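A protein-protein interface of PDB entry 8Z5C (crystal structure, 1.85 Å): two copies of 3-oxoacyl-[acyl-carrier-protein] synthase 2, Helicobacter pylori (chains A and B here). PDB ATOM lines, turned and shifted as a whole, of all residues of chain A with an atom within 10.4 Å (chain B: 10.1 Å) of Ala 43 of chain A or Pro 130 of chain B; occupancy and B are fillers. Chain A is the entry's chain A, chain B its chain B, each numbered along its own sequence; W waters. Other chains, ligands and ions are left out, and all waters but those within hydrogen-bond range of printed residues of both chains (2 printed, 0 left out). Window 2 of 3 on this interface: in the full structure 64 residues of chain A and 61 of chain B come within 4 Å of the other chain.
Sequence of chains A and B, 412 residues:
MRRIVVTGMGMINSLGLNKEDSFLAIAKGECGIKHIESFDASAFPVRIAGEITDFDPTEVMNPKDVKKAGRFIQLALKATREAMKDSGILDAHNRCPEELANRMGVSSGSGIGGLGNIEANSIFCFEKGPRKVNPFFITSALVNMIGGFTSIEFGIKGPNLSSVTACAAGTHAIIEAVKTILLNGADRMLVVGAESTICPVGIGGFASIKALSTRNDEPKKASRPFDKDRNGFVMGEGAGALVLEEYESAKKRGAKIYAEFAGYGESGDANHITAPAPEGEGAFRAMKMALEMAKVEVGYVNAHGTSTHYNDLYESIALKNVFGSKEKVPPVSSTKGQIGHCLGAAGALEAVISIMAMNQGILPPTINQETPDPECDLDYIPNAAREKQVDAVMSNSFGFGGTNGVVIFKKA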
ATOM      1  N   ILE A  36      13.369   1.292  -1.516  1.00  0.00           N
ATOM      2  CA  ILE A  36      14.034   0.001  -1.720  1.00  0.00           C
ATOM      3  C   ILE A  36      14.828  -0.425  -0.490  1.00  0.00           C
ATOM      4  O   ILE A  36      15.652   0.333   0.044  1.00  0.00           O
ATOM      5  CB  ILE A  36      14.921   0.061  -2.972  1.00  0.00           C
ATOM      6  CG1 ILE A  36      14.025   0.232  -4.213  1.00  0.00           C
ATOM      7  CG2 ILE A  36      15.812  -1.177  -3.061  1.00  0.00           C
ATOM      8  CD1 ILE A  36      14.771   0.391  -5.528  1.00  0.00           C
ATOM      9  N   PHE A  39      18.171  -4.042  -1.917  1.00  0.00           N
ATOM     10  CA  PHE A  39      19.573  -3.750  -2.219  1.00  0.00           C
ATOM     11  C   PHE A  39      19.847  -2.303  -1.816  1.00  0.00           C
ATOM     12  O   PHE A  39      18.951  -1.577  -1.374  1.00  0.00           O
ATOM     13  CB  PHE A  39      19.931  -4.031  -3.698  1.00  0.00           C
ATOM     14  CG  PHE A  39      19.317  -3.069  -4.691  1.00  0.00           C
ATOM     15  CD1 PHE A  39      18.064  -3.328  -5.247  1.00  0.00           C
ATOM     16  CD2 PHE A  39      20.010  -1.943  -5.112  1.00  0.00           C
ATOM     17  CE1 PHE A  39      17.489  -2.454  -6.184  1.00  0.00           C
ATOM     18  CE2 PHE A  39      19.460  -1.062  -6.040  1.00  0.00           C
ATOM     19  CZ  PHE A  39      18.191  -1.320  -6.590  1.00  0.00           C
ATOM     20  N   ASP A  40      21.110  -1.900  -1.921  1.00  0.00           N
ATOM     21  CA  ASP A  40      21.511  -0.545  -1.542  1.00  0.00           C
ATOM     22  C   ASP A  40      21.283   0.372  -2.731  1.00  0.00           C
ATOM     23  O   ASP A  40      22.155   0.545  -3.585  1.00  0.00           O
ATOM     24  CB  ASP A  40      22.967  -0.512  -1.088  1.00  0.00           C
ATOM     25  CG  ASP A  40      23.452   0.903  -0.782  1.00  0.00           C
ATOM     26  OD1 ASP A  40      22.617   1.825  -0.713  1.00  0.00           O
ATOM     27  OD2 ASP A  40      24.670   1.093  -0.573  1.00  0.00           O
ATOM     28  N   ALA A  41      20.109   0.999  -2.764  1.00  0.00           N
ATOM     29  CA  ALA A  41      19.746   1.916  -3.833  1.00  0.00           C
ATOM     30  C   ALA A  41      20.049   3.364  -3.484  1.00  0.00           C
ATOM     31  O   ALA A  41      19.579   4.263  -4.186  1.00  0.00           O
ATOM     32  CB  ALA A  41      18.255   1.774  -4.170  1.00  0.00           C
ATOM     33  N   SER A  42      20.819   3.615  -2.417  1.00  0.00           N
ATOM     34  CA  SER A  42      20.964   4.983  -1.918  1.00  0.00           C
ATOM     35  C   SER A  42      21.574   5.919  -2.954  1.00  0.00           C
ATOM     36  O   SER A  42      21.234   7.106  -2.986  1.00  0.00           O
ATOM     37  CB  SER A  42      21.811   4.995  -0.644  1.00  0.00           C
ATOM     38  OG  SER A  42      23.104   4.465  -0.884  1.00  0.00           O
ATOM     39  N   ALA A  43      22.464   5.413  -3.810  1.00  0.00           N
ATOM     40  CA  ALA A  43      23.112   6.225  -4.842  1.00  0.00           C
ATOM     41  C   ALA A  43      22.434   6.153  -6.209  1.00  0.00           C
ATOM     42  O   ALA A  43      22.933   6.764  -7.163  1.00  0.00           O
ATOM     43  CB  ALA A  43      24.577   5.813  -5.001  1.00  0.00           C
ATOM     44  N   PHE A  44      21.312   5.444  -6.331  1.00  0.00           N
ATOM     45  CA  PHE A  44      20.608   5.331  -7.608  1.00  0.00           C
ATOM     46  C   PHE A  44      19.679   6.517  -7.874  1.00  0.00           C
ATOM     47  O   PHE A  44      19.221   7.192  -6.945  1.00  0.00           O
ATOM     48  CB  PHE A  44      19.800   4.033  -7.638  1.00  0.00           C
ATOM     49  CG  PHE A  44      20.634   2.804  -7.881  1.00  0.00           C
ATOM     50  CD1 PHE A  44      21.700   2.477  -7.043  1.00  0.00           C
ATOM     51  CD2 PHE A  44      20.362   1.987  -8.960  1.00  0.00           C
ATOM     52  CE1 PHE A  44      22.471   1.352  -7.278  1.00  0.00           C
ATOM     53  CE2 PHE A  44      21.125   0.852  -9.203  1.00  0.00           C
ATOM     54  CZ  PHE A  44      22.185   0.535  -8.353  1.00  0.00           C
ATOM     55  N   PRO A  45      19.346   6.772  -9.147  1.00  0.00           N
ATOM     56  CA  PRO A  45      18.360   7.823  -9.444  1.00  0.00           C
ATOM     57  C   PRO A  45      16.936   7.417  -9.114  1.00  0.00           C
ATOM     58  O   PRO A  45      16.070   8.296  -8.992  1.00  0.00           O
ATOM     59  CB  PRO A  45      18.531   8.047 -10.953  1.00  0.00           C
ATOM     60  CG  PRO A  45      18.998   6.725 -11.455  1.00  0.00           C
ATOM     61  CD  PRO A  45      19.857   6.132 -10.373  1.00  0.00           C
ATOM     62  N   VAL A  46      16.661   6.120  -8.992  1.00  0.00           N
ATOM     63  CA  VAL A  46      15.365   5.613  -8.547  1.00  0.00           C
ATOM     64  C   VAL A  46      15.606   4.777  -7.301  1.00  0.00           C
ATOM     65  O   VAL A  46      16.484   3.908  -7.299  1.00  0.00           O
ATOM     66  CB  VAL A  46      14.665   4.778  -9.634  1.00  0.00           C
ATOM     67  CG1 VAL A  46      13.368   4.200  -9.099  1.00  0.00           C
ATOM     68  CG2 VAL A  46      14.408   5.635 -10.891  1.00  0.00           C
ATOM     69  N   ARG A  47      14.853   5.063  -6.231  1.00  0.00           N
ATOM     70  CA  ARG A  47      15.147   4.477  -4.928  1.00  0.00           C
ATOM     71  C   ARG A  47      13.907   3.852  -4.295  1.00  0.00           C
ATOM     72  O   ARG A  47      13.906   3.562  -3.085  1.00  0.00           O
ATOM     73  CB  ARG A  47      15.756   5.543  -4.016  1.00  0.00           C
ATOM     74  CG  ARG A  47      17.077   6.060  -4.578  1.00  0.00           C
ATOM     75  CD  ARG A  47      17.809   6.970  -3.602  1.00  0.00           C
ATOM     76  NE  ARG A  47      17.091   8.203  -3.325  1.00  0.00           N
ATOM     77  CZ  ARG A  47      17.163   9.290  -4.087  1.00  0.00           C
ATOM     78  NH1 ARG A  47      17.880   9.309  -5.205  1.00  0.00           N
ATOM     79  NH2 ARG A  47      16.509  10.388  -3.717  1.00  0.00           N
ATOM     80  N   ILE A  48      12.865   3.619  -5.101  1.00  0.00           N
ATOM     81  CA  ILE A  48      11.571   3.124  -4.651  1.00  0.00           C
ATOM     82  C   ILE A  48      11.144   1.953  -5.531  1.00  0.00           C
ATOM     83  O   ILE A  48      11.542   1.841  -6.692  1.00  0.00           O
ATOM     84  CB  ILE A  48      10.497   4.226  -4.696  1.00  0.00           C
ATOM     85  CG1 ILE A  48      10.396   4.771  -6.119  1.00  0.00           C
ATOM     86  CG2 ILE A  48      10.829   5.351  -3.714  1.00  0.00           C
ATOM     87  CD1 ILE A  48       9.194   5.700  -6.339  1.00  0.00           C
ATOM     88  N   GLU A 119      22.735 -11.371 -12.604  1.00  0.00           N
ATOM     89  CA  GLU A 119      23.623 -10.361 -12.023  1.00  0.00           C
ATOM     90  C   GLU A 119      24.695 -10.931 -11.124  1.00  0.00           C
ATOM     91  O   GLU A 119      25.893 -10.671 -11.299  1.00  0.00           O
ATOM     92  CB  GLU A 119      22.850  -9.369 -11.156  1.00  0.00           C
ATOM     93  CG  GLU A 119      23.422  -7.985 -11.136  1.00  0.00           C
ATOM     94  CD  GLU A 119      22.506  -7.009 -10.456  1.00  0.00           C
ATOM     95  OE1 GLU A 119      21.642  -7.460  -9.664  1.00  0.00           O
ATOM     96  OE2 GLU A 119      22.708  -5.804 -10.644  1.00  0.00           O
ATOM     97  N   CYS A 199      16.570  -5.207  -8.434  1.00  0.00           N
ATOM     98  CA  CYS A 199      17.995  -5.431  -8.243  1.00  0.00           C
ATOM     99  C   CYS A 199      18.716  -4.301  -8.955  1.00  0.00           C
ATOM    100  O   CYS A 199      18.105  -3.569  -9.741  1.00  0.00           O
ATOM    101  CB  CYS A 199      18.416  -6.803  -8.801  1.00  0.00           C
ATOM    102  SG  CYS A 199      18.234  -6.989 -10.618  1.00  0.00           S
ATOM    103  N   PRO A 200      20.020  -4.112  -8.690  1.00  0.00           N
ATOM    104  CA  PRO A 200      20.716  -2.968  -9.306  1.00  0.00           C
ATOM    105  C   PRO A 200      20.590  -2.899 -10.832  1.00  0.00           C
ATOM    106  O   PRO A 200      20.322  -1.818 -11.378  1.00  0.00           O
ATOM    107  CB  PRO A 200      22.173  -3.183  -8.853  1.00  0.00           C
ATOM    108  CG  PRO A 200      22.043  -3.863  -7.532  1.00  0.00           C
ATOM    109  CD  PRO A 200      20.889  -4.821  -7.726  1.00  0.00           C
ATOM    110  N   VAL A 201      20.782  -4.012 -11.549  1.00  0.00           N
ATOM    111  CA  VAL A 201      20.793  -3.883 -13.006  1.00  0.00           C
ATOM    112  C   VAL A 201      19.356  -3.718 -13.507  1.00  0.00           C
ATOM    113  O   VAL A 201      19.126  -3.096 -14.553  1.00  0.00           O
ATOM    114  CB  VAL A 201      21.502  -5.067 -13.706  1.00  0.00           C
ATOM    115  CG1 VAL A 201      20.915  -6.417 -13.332  1.00  0.00           C
ATOM    116  CG2 VAL A 201      21.589  -4.868 -15.197  1.00  0.00           C
ATOM    117  N   GLY A 202      18.368  -4.219 -12.758  1.00  0.00           N
ATOM    118  CA  GLY A 202      16.977  -4.007 -13.144  1.00  0.00           C
ATOM    119  C   GLY A 202      16.535  -2.561 -12.999  1.00  0.00           C
ATOM    120  O   GLY A 202      16.046  -1.945 -13.958  1.00  0.00           O
ATOM    121  N   ILE A 203      16.703  -1.996 -11.797  1.00  0.00           N
ATOM    122  CA  ILE A 203      16.353  -0.595 -11.568  1.00  0.00           C
ATOM    123  C   ILE A 203      17.214   0.314 -12.434  1.00  0.00           C
ATOM    124  O   ILE A 203      16.716   1.259 -13.046  1.00  0.00           O
ATOM    125  CB  ILE A 203      16.491  -0.231 -10.076  1.00  0.00           C
ATOM    126  CG1 ILE A 203      15.482  -1.021  -9.231  1.00  0.00           C
ATOM    127  CG2 ILE A 203      16.345   1.285  -9.863  1.00  0.00           C
ATOM    128  CD1 ILE A 203      14.027  -0.565  -9.416  1.00  0.00           C
ATOM    129  N   GLY A 204      18.527   0.055 -12.480  1.00  0.00           N
ATOM    130  CA  GLY A 204      19.393   0.886 -13.301  1.00  0.00           C
ATOM    131  C   GLY A 204      19.023   0.818 -14.769  1.00  0.00           C
ATOM    132  O   GLY A 204      19.070   1.823 -15.482  1.00  0.00           O
ATOM    133  N   GLY A 205      18.609  -0.361 -15.231  1.00  0.00           N
ATOM    134  CA  GLY A 205      18.342  -0.528 -16.646  1.00  0.00           C
ATOM    135  C   GLY A 205      17.097   0.216 -17.081  1.00  0.00           C
ATOM    136  O   GLY A 205      17.090   0.896 -18.106  1.00  0.00           O
ATOM    137  N   PHE A 206      16.027   0.104 -16.300  1.00  0.00           N
ATOM    138  CA  PHE A 206      14.819   0.841 -16.647  1.00  0.00           C
ATOM    139  C   PHE A 206      14.963   2.329 -16.360  1.00  0.00           C
ATOM    140  O   PHE A 206      14.305   3.149 -17.011  1.00  0.00           O
ATOM    141  CB  PHE A 206      13.618   0.228 -15.929  1.00  0.00           C
ATOM    142  CG  PHE A 206      13.123  -1.030 -16.599  1.00  0.00           C
ATOM    143  CD1 PHE A 206      12.417  -0.962 -17.793  1.00  0.00           C
ATOM    144  CD2 PHE A 206      13.430  -2.282 -16.074  1.00  0.00           C
ATOM    145  CE1 PHE A 206      11.992  -2.135 -18.442  1.00  0.00           C
ATOM    146  CE2 PHE A 206      13.008  -3.451 -16.707  1.00  0.00           C
ATOM    147  CZ  PHE A 206      12.291  -3.382 -17.886  1.00  0.00           C
ATOM    148  N   ALA A 207      15.844   2.710 -15.427  1.00  0.00           N
ATOM    149  CA  ALA A 207      16.062   4.138 -15.212  1.00  0.00           C
ATOM    150  C   ALA A 207      16.845   4.747 -16.367  1.00  0.00           C
ATOM    151  O   ALA A 207      16.599   5.893 -16.753  1.00  0.00           O
ATOM    152  CB  ALA A 207      16.792   4.375 -13.887  1.00  0.00           C
ATOM    153  N   SER A 208      17.787   3.994 -16.944  1.00  0.00           N
ATOM    154  CA  SER A 208      18.603   4.571 -18.008  1.00  0.00           C
ATOM    155  C   SER A 208      17.836   4.711 -19.320  1.00  0.00           C
ATOM    156  O   SER A 208      18.228   5.518 -20.168  1.00  0.00           O
ATOM    157  CB  SER A 208      19.884   3.744 -18.208  1.00  0.00           C
ATOM    158  OG  SER A 208      19.592   2.468 -18.730  1.00  0.00           O
ATOM    159  N   ILE A 209      16.750   3.964 -19.512  1.00  0.00           N
ATOM    160  CA  ILE A 209      15.892   4.199 -20.669  1.00  0.00           C
ATOM    161  C   ILE A 209      14.797   5.184 -20.288  1.00  0.00           C
ATOM    162  O   ILE A 209      13.839   5.372 -21.045  1.00  0.00           O
ATOM    163  CB  ILE A 209      15.295   2.892 -21.222  1.00  0.00           C
ATOM    164  CG1 ILE A 209      14.317   2.278 -20.218  1.00  0.00           C
ATOM    165  CG2 ILE A 209      16.394   1.922 -21.597  1.00  0.00           C
ATOM    166  CD1 ILE A 209      13.455   1.158 -20.800  1.00  0.00           C
ATOM    167  N   LYS A 210      14.930   5.808 -19.112  1.00  0.00           N
ATOM    168  CA  LYS A 210      14.026   6.875 -18.647  1.00  0.00           C
ATOM    169  C   LYS A 210      12.585   6.405 -18.444  1.00  0.00           C
ATOM    170  O   LYS A 210      11.642   7.186 -18.588  1.00  0.00           O
ATOM    171  CB  LYS A 210      14.036   8.077 -19.601  1.00  0.00           C
ATOM    172  CG  LYS A 210      14.989   9.197 -19.230  1.00  0.00           C
ATOM    173  CD  LYS A 210      16.408   8.716 -19.036  1.00  0.00           C
ATOM    174  CE  LYS A 210      17.093   9.474 -17.900  1.00  0.00           C
ATOM    175  NZ  LYS A 210      18.318   8.748 -17.432  1.00  0.00           N
ATOM    176  N   ASN A 216      11.232  10.096  -5.681  1.00  0.00           N
ATOM    177  CA  ASN A 216      11.713   9.293  -4.566  1.00  0.00           C
ATOM    178  C   ASN A 216      11.268   9.801  -3.204  1.00  0.00           C
ATOM    179  O   ASN A 216      11.308   9.027  -2.247  1.00  0.00           O
ATOM    180  CB  ASN A 216      13.236   9.208  -4.599  1.00  0.00           C
ATOM    181  CG  ASN A 216      13.737   8.542  -5.854  1.00  0.00           C
ATOM    182  OD1 ASN A 216      13.389   7.397  -6.121  1.00  0.00           O
ATOM    183  ND2 ASN A 216      14.585   9.230  -6.607  1.00  0.00           N
ATOM    184  N   ASN B 121      26.260  -5.376 -18.342  1.00  0.00           N
ATOM    185  CA  ASN B 121      25.721  -4.264 -17.573  1.00  0.00           C
ATOM    186  C   ASN B 121      25.762  -4.554 -16.076  1.00  0.00           C
ATOM    187  O   ASN B 121      25.934  -3.633 -15.265  1.00  0.00           O
ATOM    188  CB  ASN B 121      24.306  -3.954 -18.052  1.00  0.00           C
ATOM    189  CG  ASN B 121      24.308  -3.194 -19.365  1.00  0.00           C
ATOM    190  OD1 ASN B 121      24.517  -1.993 -19.396  1.00  0.00           O
ATOM    191  ND2 ASN B 121      24.116  -3.909 -20.457  1.00  0.00           N
ATOM    192  N   SER B 122      25.651  -5.827 -15.700  1.00  0.00           N
ATOM    193  CA  SER B 122      25.804  -6.216 -14.300  1.00  0.00           C
ATOM    194  C   SER B 122      27.202  -5.873 -13.808  1.00  0.00           C
ATOM    195  O   SER B 122      27.377  -5.276 -12.736  1.00  0.00           O
ATOM    196  CB  SER B 122      25.555  -7.719 -14.165  1.00  0.00           C
ATOM    197  OG  SER B 122      24.184  -8.030 -14.404  1.00  0.00           O
ATOM    198  N   ILE B 123      28.213  -6.272 -14.587  1.00  0.00           N
ATOM    199  CA  ILE B 123      29.599  -5.970 -14.253  1.00  0.00           C
ATOM    200  C   ILE B 123      29.800  -4.466 -14.204  1.00  0.00           C
ATOM    201  O   ILE B 123      30.450  -3.931 -13.297  1.00  0.00           O
ATOM    202  CB  ILE B 123      30.546  -6.638 -15.272  1.00  0.00           C
ATOM    203  CG1 ILE B 123      30.497  -8.157 -15.133  1.00  0.00           C
ATOM    204  CG2 ILE B 123      31.994  -6.136 -15.098  1.00  0.00           C
ATOM    205  CD1 ILE B 123      31.101  -8.887 -16.330  1.00  0.00           C
ATOM    206  N   PHE B 124      29.203  -3.750 -15.147  1.00  0.00           N
ATOM    207  CA  PHE B 124      29.524  -2.337 -15.241  1.00  0.00           C
ATOM    208  C   PHE B 124      28.878  -1.579 -14.081  1.00  0.00           C
ATOM    209  O   PHE B 124      29.517  -0.720 -13.459  1.00  0.00           O
ATOM    210  CB  PHE B 124      29.098  -1.831 -16.623  1.00  0.00           C
ATOM    211  CG  PHE B 124      29.314  -0.371 -16.839  1.00  0.00           C
ATOM    212  CD1 PHE B 124      28.446   0.586 -16.330  1.00  0.00           C
ATOM    213  CD2 PHE B 124      30.425   0.046 -17.564  1.00  0.00           C
ATOM    214  CE1 PHE B 124      28.686   1.939 -16.554  1.00  0.00           C
ATOM    215  CE2 PHE B 124      30.672   1.389 -17.790  1.00  0.00           C
ATOM    216  CZ  PHE B 124      29.805   2.338 -17.280  1.00  0.00           C
ATOM    217  N   CYS B 125      27.675  -1.970 -13.672  1.00  0.00           N
ATOM    218  CA  CYS B 125      27.011  -1.343 -12.495  1.00  0.00           C
ATOM    219  C   CYS B 125      27.843  -1.638 -11.248  1.00  0.00           C
ATOM    220  O   CYS B 125      27.970  -0.757 -10.420  1.00  0.00           O
ATOM    221  CB  CYS B 125      25.587  -1.863 -12.321  1.00  0.00           C
ATOM    222  SG  CYS B 125      24.608  -0.983 -11.078  1.00  0.00           S
ATOM    223  N   PHE B 126      28.382  -2.843 -11.153  1.00  0.00           N
ATOM    224  CA  PHE B 126      29.144  -3.259  -9.954  1.00  0.00           C
ATOM    225  C   PHE B 126      30.436  -2.454  -9.845  1.00  0.00           C
ATOM    226  O   PHE B 126      30.782  -2.060  -8.751  1.00  0.00           O
ATOM    227  CB  PHE B 126      29.458  -4.738 -10.033  1.00  0.00           C
ATOM    228  CG  PHE B 126      30.345  -5.259  -8.940  1.00  0.00           C
ATOM    229  CD1 PHE B 126      29.898  -5.317  -7.634  1.00  0.00           C
ATOM    230  CD2 PHE B 126      31.632  -5.677  -9.222  1.00  0.00           C
ATOM    231  CE1 PHE B 126      30.723  -5.796  -6.633  1.00  0.00           C
ATOM    232  CE2 PHE B 126      32.454  -6.154  -8.218  1.00  0.00           C
ATOM    233  CZ  PHE B 126      31.998  -6.211  -6.928  1.00  0.00           C
ATOM    234  N   GLU B 127      31.093  -2.240 -10.966  1.00  0.00           N
ATOM    235  CA  GLU B 127      32.394  -1.527 -10.969  1.00  0.00           C
ATOM    236  C   GLU B 127      32.237  -0.003 -10.963  1.00  0.00           C
ATOM    237  O   GLU B 127      32.956   0.630 -10.204  1.00  0.00           O
ATOM    238  CB  GLU B 127      33.163  -1.890 -12.234  1.00  0.00           C
ATOM    239  CG  GLU B 127      33.657  -3.321 -12.312  1.00  0.00           C
ATOM    240  CD  GLU B 127      34.760  -3.515 -13.339  1.00  0.00           C
ATOM    241  OE1 GLU B 127      34.492  -3.351 -14.542  1.00  0.00           O
ATOM    242  OE2 GLU B 127      35.889  -3.809 -12.932  1.00  0.00           O
ATOM    243  N   LYS B 128      31.290   0.547 -11.699  1.00  0.00           N
ATOM    244  CA  LYS B 128      31.209   2.006 -11.915  1.00  0.00           C
ATOM    245  C   LYS B 128      29.939   2.644 -11.353  1.00  0.00           C
ATOM    246  O   LYS B 128      29.793   3.851 -11.463  1.00  0.00           O
ATOM    247  CB  LYS B 128      31.299   2.205 -13.427  1.00  0.00           C
ATOM    248  CG  LYS B 128      32.528   1.574 -14.054  1.00  0.00           C
ATOM    249  CD  LYS B 128      33.050   2.312 -15.246  1.00  0.00           C
ATOM    250  CE  LYS B 128      34.509   2.004 -15.494  1.00  0.00           C
ATOM    251  NZ  LYS B 128      34.766   0.548 -15.459  1.00  0.00           N
ATOM    252  N   GLY B 129      29.036   1.822 -10.844  1.00  0.00           N
ATOM    253  CA  GLY B 129      27.830   2.377 -10.241  1.00  0.00           C
ATOM    254  C   GLY B 129      26.694   2.609 -11.196  1.00  0.00           C
ATOM    255  O   GLY B 129      26.833   2.341 -12.387  1.00  0.00           O
ATOM    256  N   PRO B 130      25.533   3.040 -10.672  1.00  0.00           N
ATOM    257  CA  PRO B 130      24.344   3.223 -11.490  1.00  0.00           C
ATOM    258  C   PRO B 130      24.399   4.249 -12.650  1.00  0.00           C
ATOM    259  O   PRO B 130      23.714   3.993 -13.598  1.00  0.00           O
ATOM    260  CB  PRO B 130      23.357   3.740 -10.435  1.00  0.00           C
ATOM    261  CG  PRO B 130      24.190   4.305  -9.328  1.00  0.00           C
ATOM    262  CD  PRO B 130      25.342   3.338  -9.257  1.00  0.00           C
ATOM    263  N   ASN B 134      25.690   2.975 -19.296  1.00  0.00           N
ATOM    264  CA  ASN B 134      25.725   1.498 -19.371  1.00  0.00           C
ATOM    265  C   ASN B 134      26.103   0.998 -20.759  1.00  0.00           C
ATOM    266  O   ASN B 134      25.697   1.578 -21.742  1.00  0.00           O
ATOM    267  CB  ASN B 134      24.386   0.919 -18.904  1.00  0.00           C
ATOM    268  CG  ASN B 134      24.151   1.093 -17.425  1.00  0.00           C
ATOM    269  OD1 ASN B 134      24.833   1.872 -16.769  1.00  0.00           O
ATOM    270  ND2 ASN B 134      23.228   0.324 -16.873  1.00  0.00           N
ATOM    271  N   PRO B 135      26.813  -0.134 -20.859  1.00  0.00           N
ATOM    272  CA  PRO B 135      27.180  -0.658 -22.165  1.00  0.00           C
ATOM    273  C   PRO B 135      25.935  -0.940 -23.021  1.00  0.00           C
ATOM    274  O   PRO B 135      25.954  -0.690 -24.157  1.00  0.00           O
ATOM    275  CB  PRO B 135      27.893  -1.970 -21.788  1.00  0.00           C
ATOM    276  CG  PRO B 135      28.429  -1.739 -20.422  1.00  0.00           C
ATOM    277  CD  PRO B 135      27.381  -0.880 -19.766  1.00  0.00           C
ATOM    278  N   PHE B 136      24.880  -1.491 -22.440  1.00  0.00           N
ATOM    279  CA  PHE B 136      23.674  -1.875 -23.213  1.00  0.00           C
ATOM    280  C   PHE B 136      22.390  -1.439 -22.514  1.00  0.00           C
ATOM    281  O   PHE B 136      22.366  -1.204 -21.314  1.00  0.00           O
ATOM    282  CB  PHE B 136      23.606  -3.381 -23.458  1.00  0.00           C
ATOM    283  CG  PHE B 136      24.840  -3.937 -24.087  1.00  0.00           C
ATOM    284  CD1 PHE B 136      25.051  -3.791 -25.443  1.00  0.00           C
ATOM    285  CD2 PHE B 136      25.839  -4.493 -23.316  1.00  0.00           C
ATOM    286  CE1 PHE B 136      26.211  -4.263 -26.033  1.00  0.00           C
ATOM    287  CE2 PHE B 136      26.984  -4.979 -23.903  1.00  0.00           C
ATOM    288  CZ  PHE B 136      27.167  -4.838 -25.256  1.00  0.00           C
HETATM  289  O   HOH W   1      25.357  -4.894 -10.619  1.00  0.00           O
HETATM  290  O   HOH W   2      20.461   4.138 -14.551  1.00  0.00           O
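Ala 41 of chain A touches none of the printed residues of chain B. Ser 42 of chain A touches none of the printed residues of chain B. Ala 43 of chain A touches one residue of chain B. Phe 44 of chain A touches just these residues of chain B: Cys 125 (3.9 Å) and Pro 130 (3.8 Å). Printed residues of chain B within 4 Å of Glu 119 of chain A: Ser 122. Of the printed residues of chain B, Pro 200 of chain A touches Cys 125. Of the printed residues of chain B, Val 201 of chain A touches Ser 122. Of the printed residues of chain A, Ser 122 of chain B touches Glu 119 and Val 201. Of chain A, only Phe 44 and Pro 200 come within 4 Å of Cys 125 of chain B. No residue of chain A comes within 4 Å of Gly 129 of chain B. Of chain A, only Ala 43 and Phe 44 come within 4 Å of Pro 130 of chain B. The nearest residue of chain B that does not touch Ala 43 of chain A is Gly 129 of chain B (6.9 Å). The nearest printed residue of chain B that does not touch Glu 119 of chain A is Cys 125 of chain B (5.2 Å).
No position is printed for both chains. Of the 6 pairs that touch across the chains among the printed residues, none has its exchanged pair printed and touching as well.
Among the printed residues, pairs that only touch across the chains: Ala 43 of chain A with Pro 130 of chain B, Phe 44 of chain A with Cys 125 of chain B, Phe 44 of chain A with Pro 130 of chain B, Glu 119 of chain A with Ser 122 of chain B, Pro 200 of chain A with Cys 125 of chain B and Val 201 of chain A with Ser 122 of chain B.
Water W1 bridges the side-chain carboxylate of Glu 119 of chain A (2.8 Å) and the backbone carbonyl oxygen of Ser 122 of chain B (3.0 Å). Water W2 lies within hydrogen-bond range of O of Gly 204 of chain A (2.9 Å) and O of Pro 130 of chain B (3.4 Å).
Printed residues of chain A that touch a printed residue of chain B: Ala 43, Phe 44, Glu 119, Pro 200 and Val 201. Hydrophobic or aromatic side chains of chain A within 4 Å of the printed part of chain B: Phe 44, Pro 200 and Val 201. Printed residues of chain B that touch a printed residue of chain A: Ser 122, Cys 125 and Pro 130.
The side-chain carboxylate (OE2) of Glu 119 of chain A lies within hydrogen-bond range of the backbone NH (N) of Val 201 of chain A (2.8 Å). The side-chain sulfur of Cys 199 of chain A sits close to the side-chain carboxylate of Glu 119 of chain A (3.6 Å). The guanidinium group (NH1) of Arg 47 of chain A lies within hydrogen-bond range of the backbone carbonyl oxygen (O) of Phe 44 of chain A.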
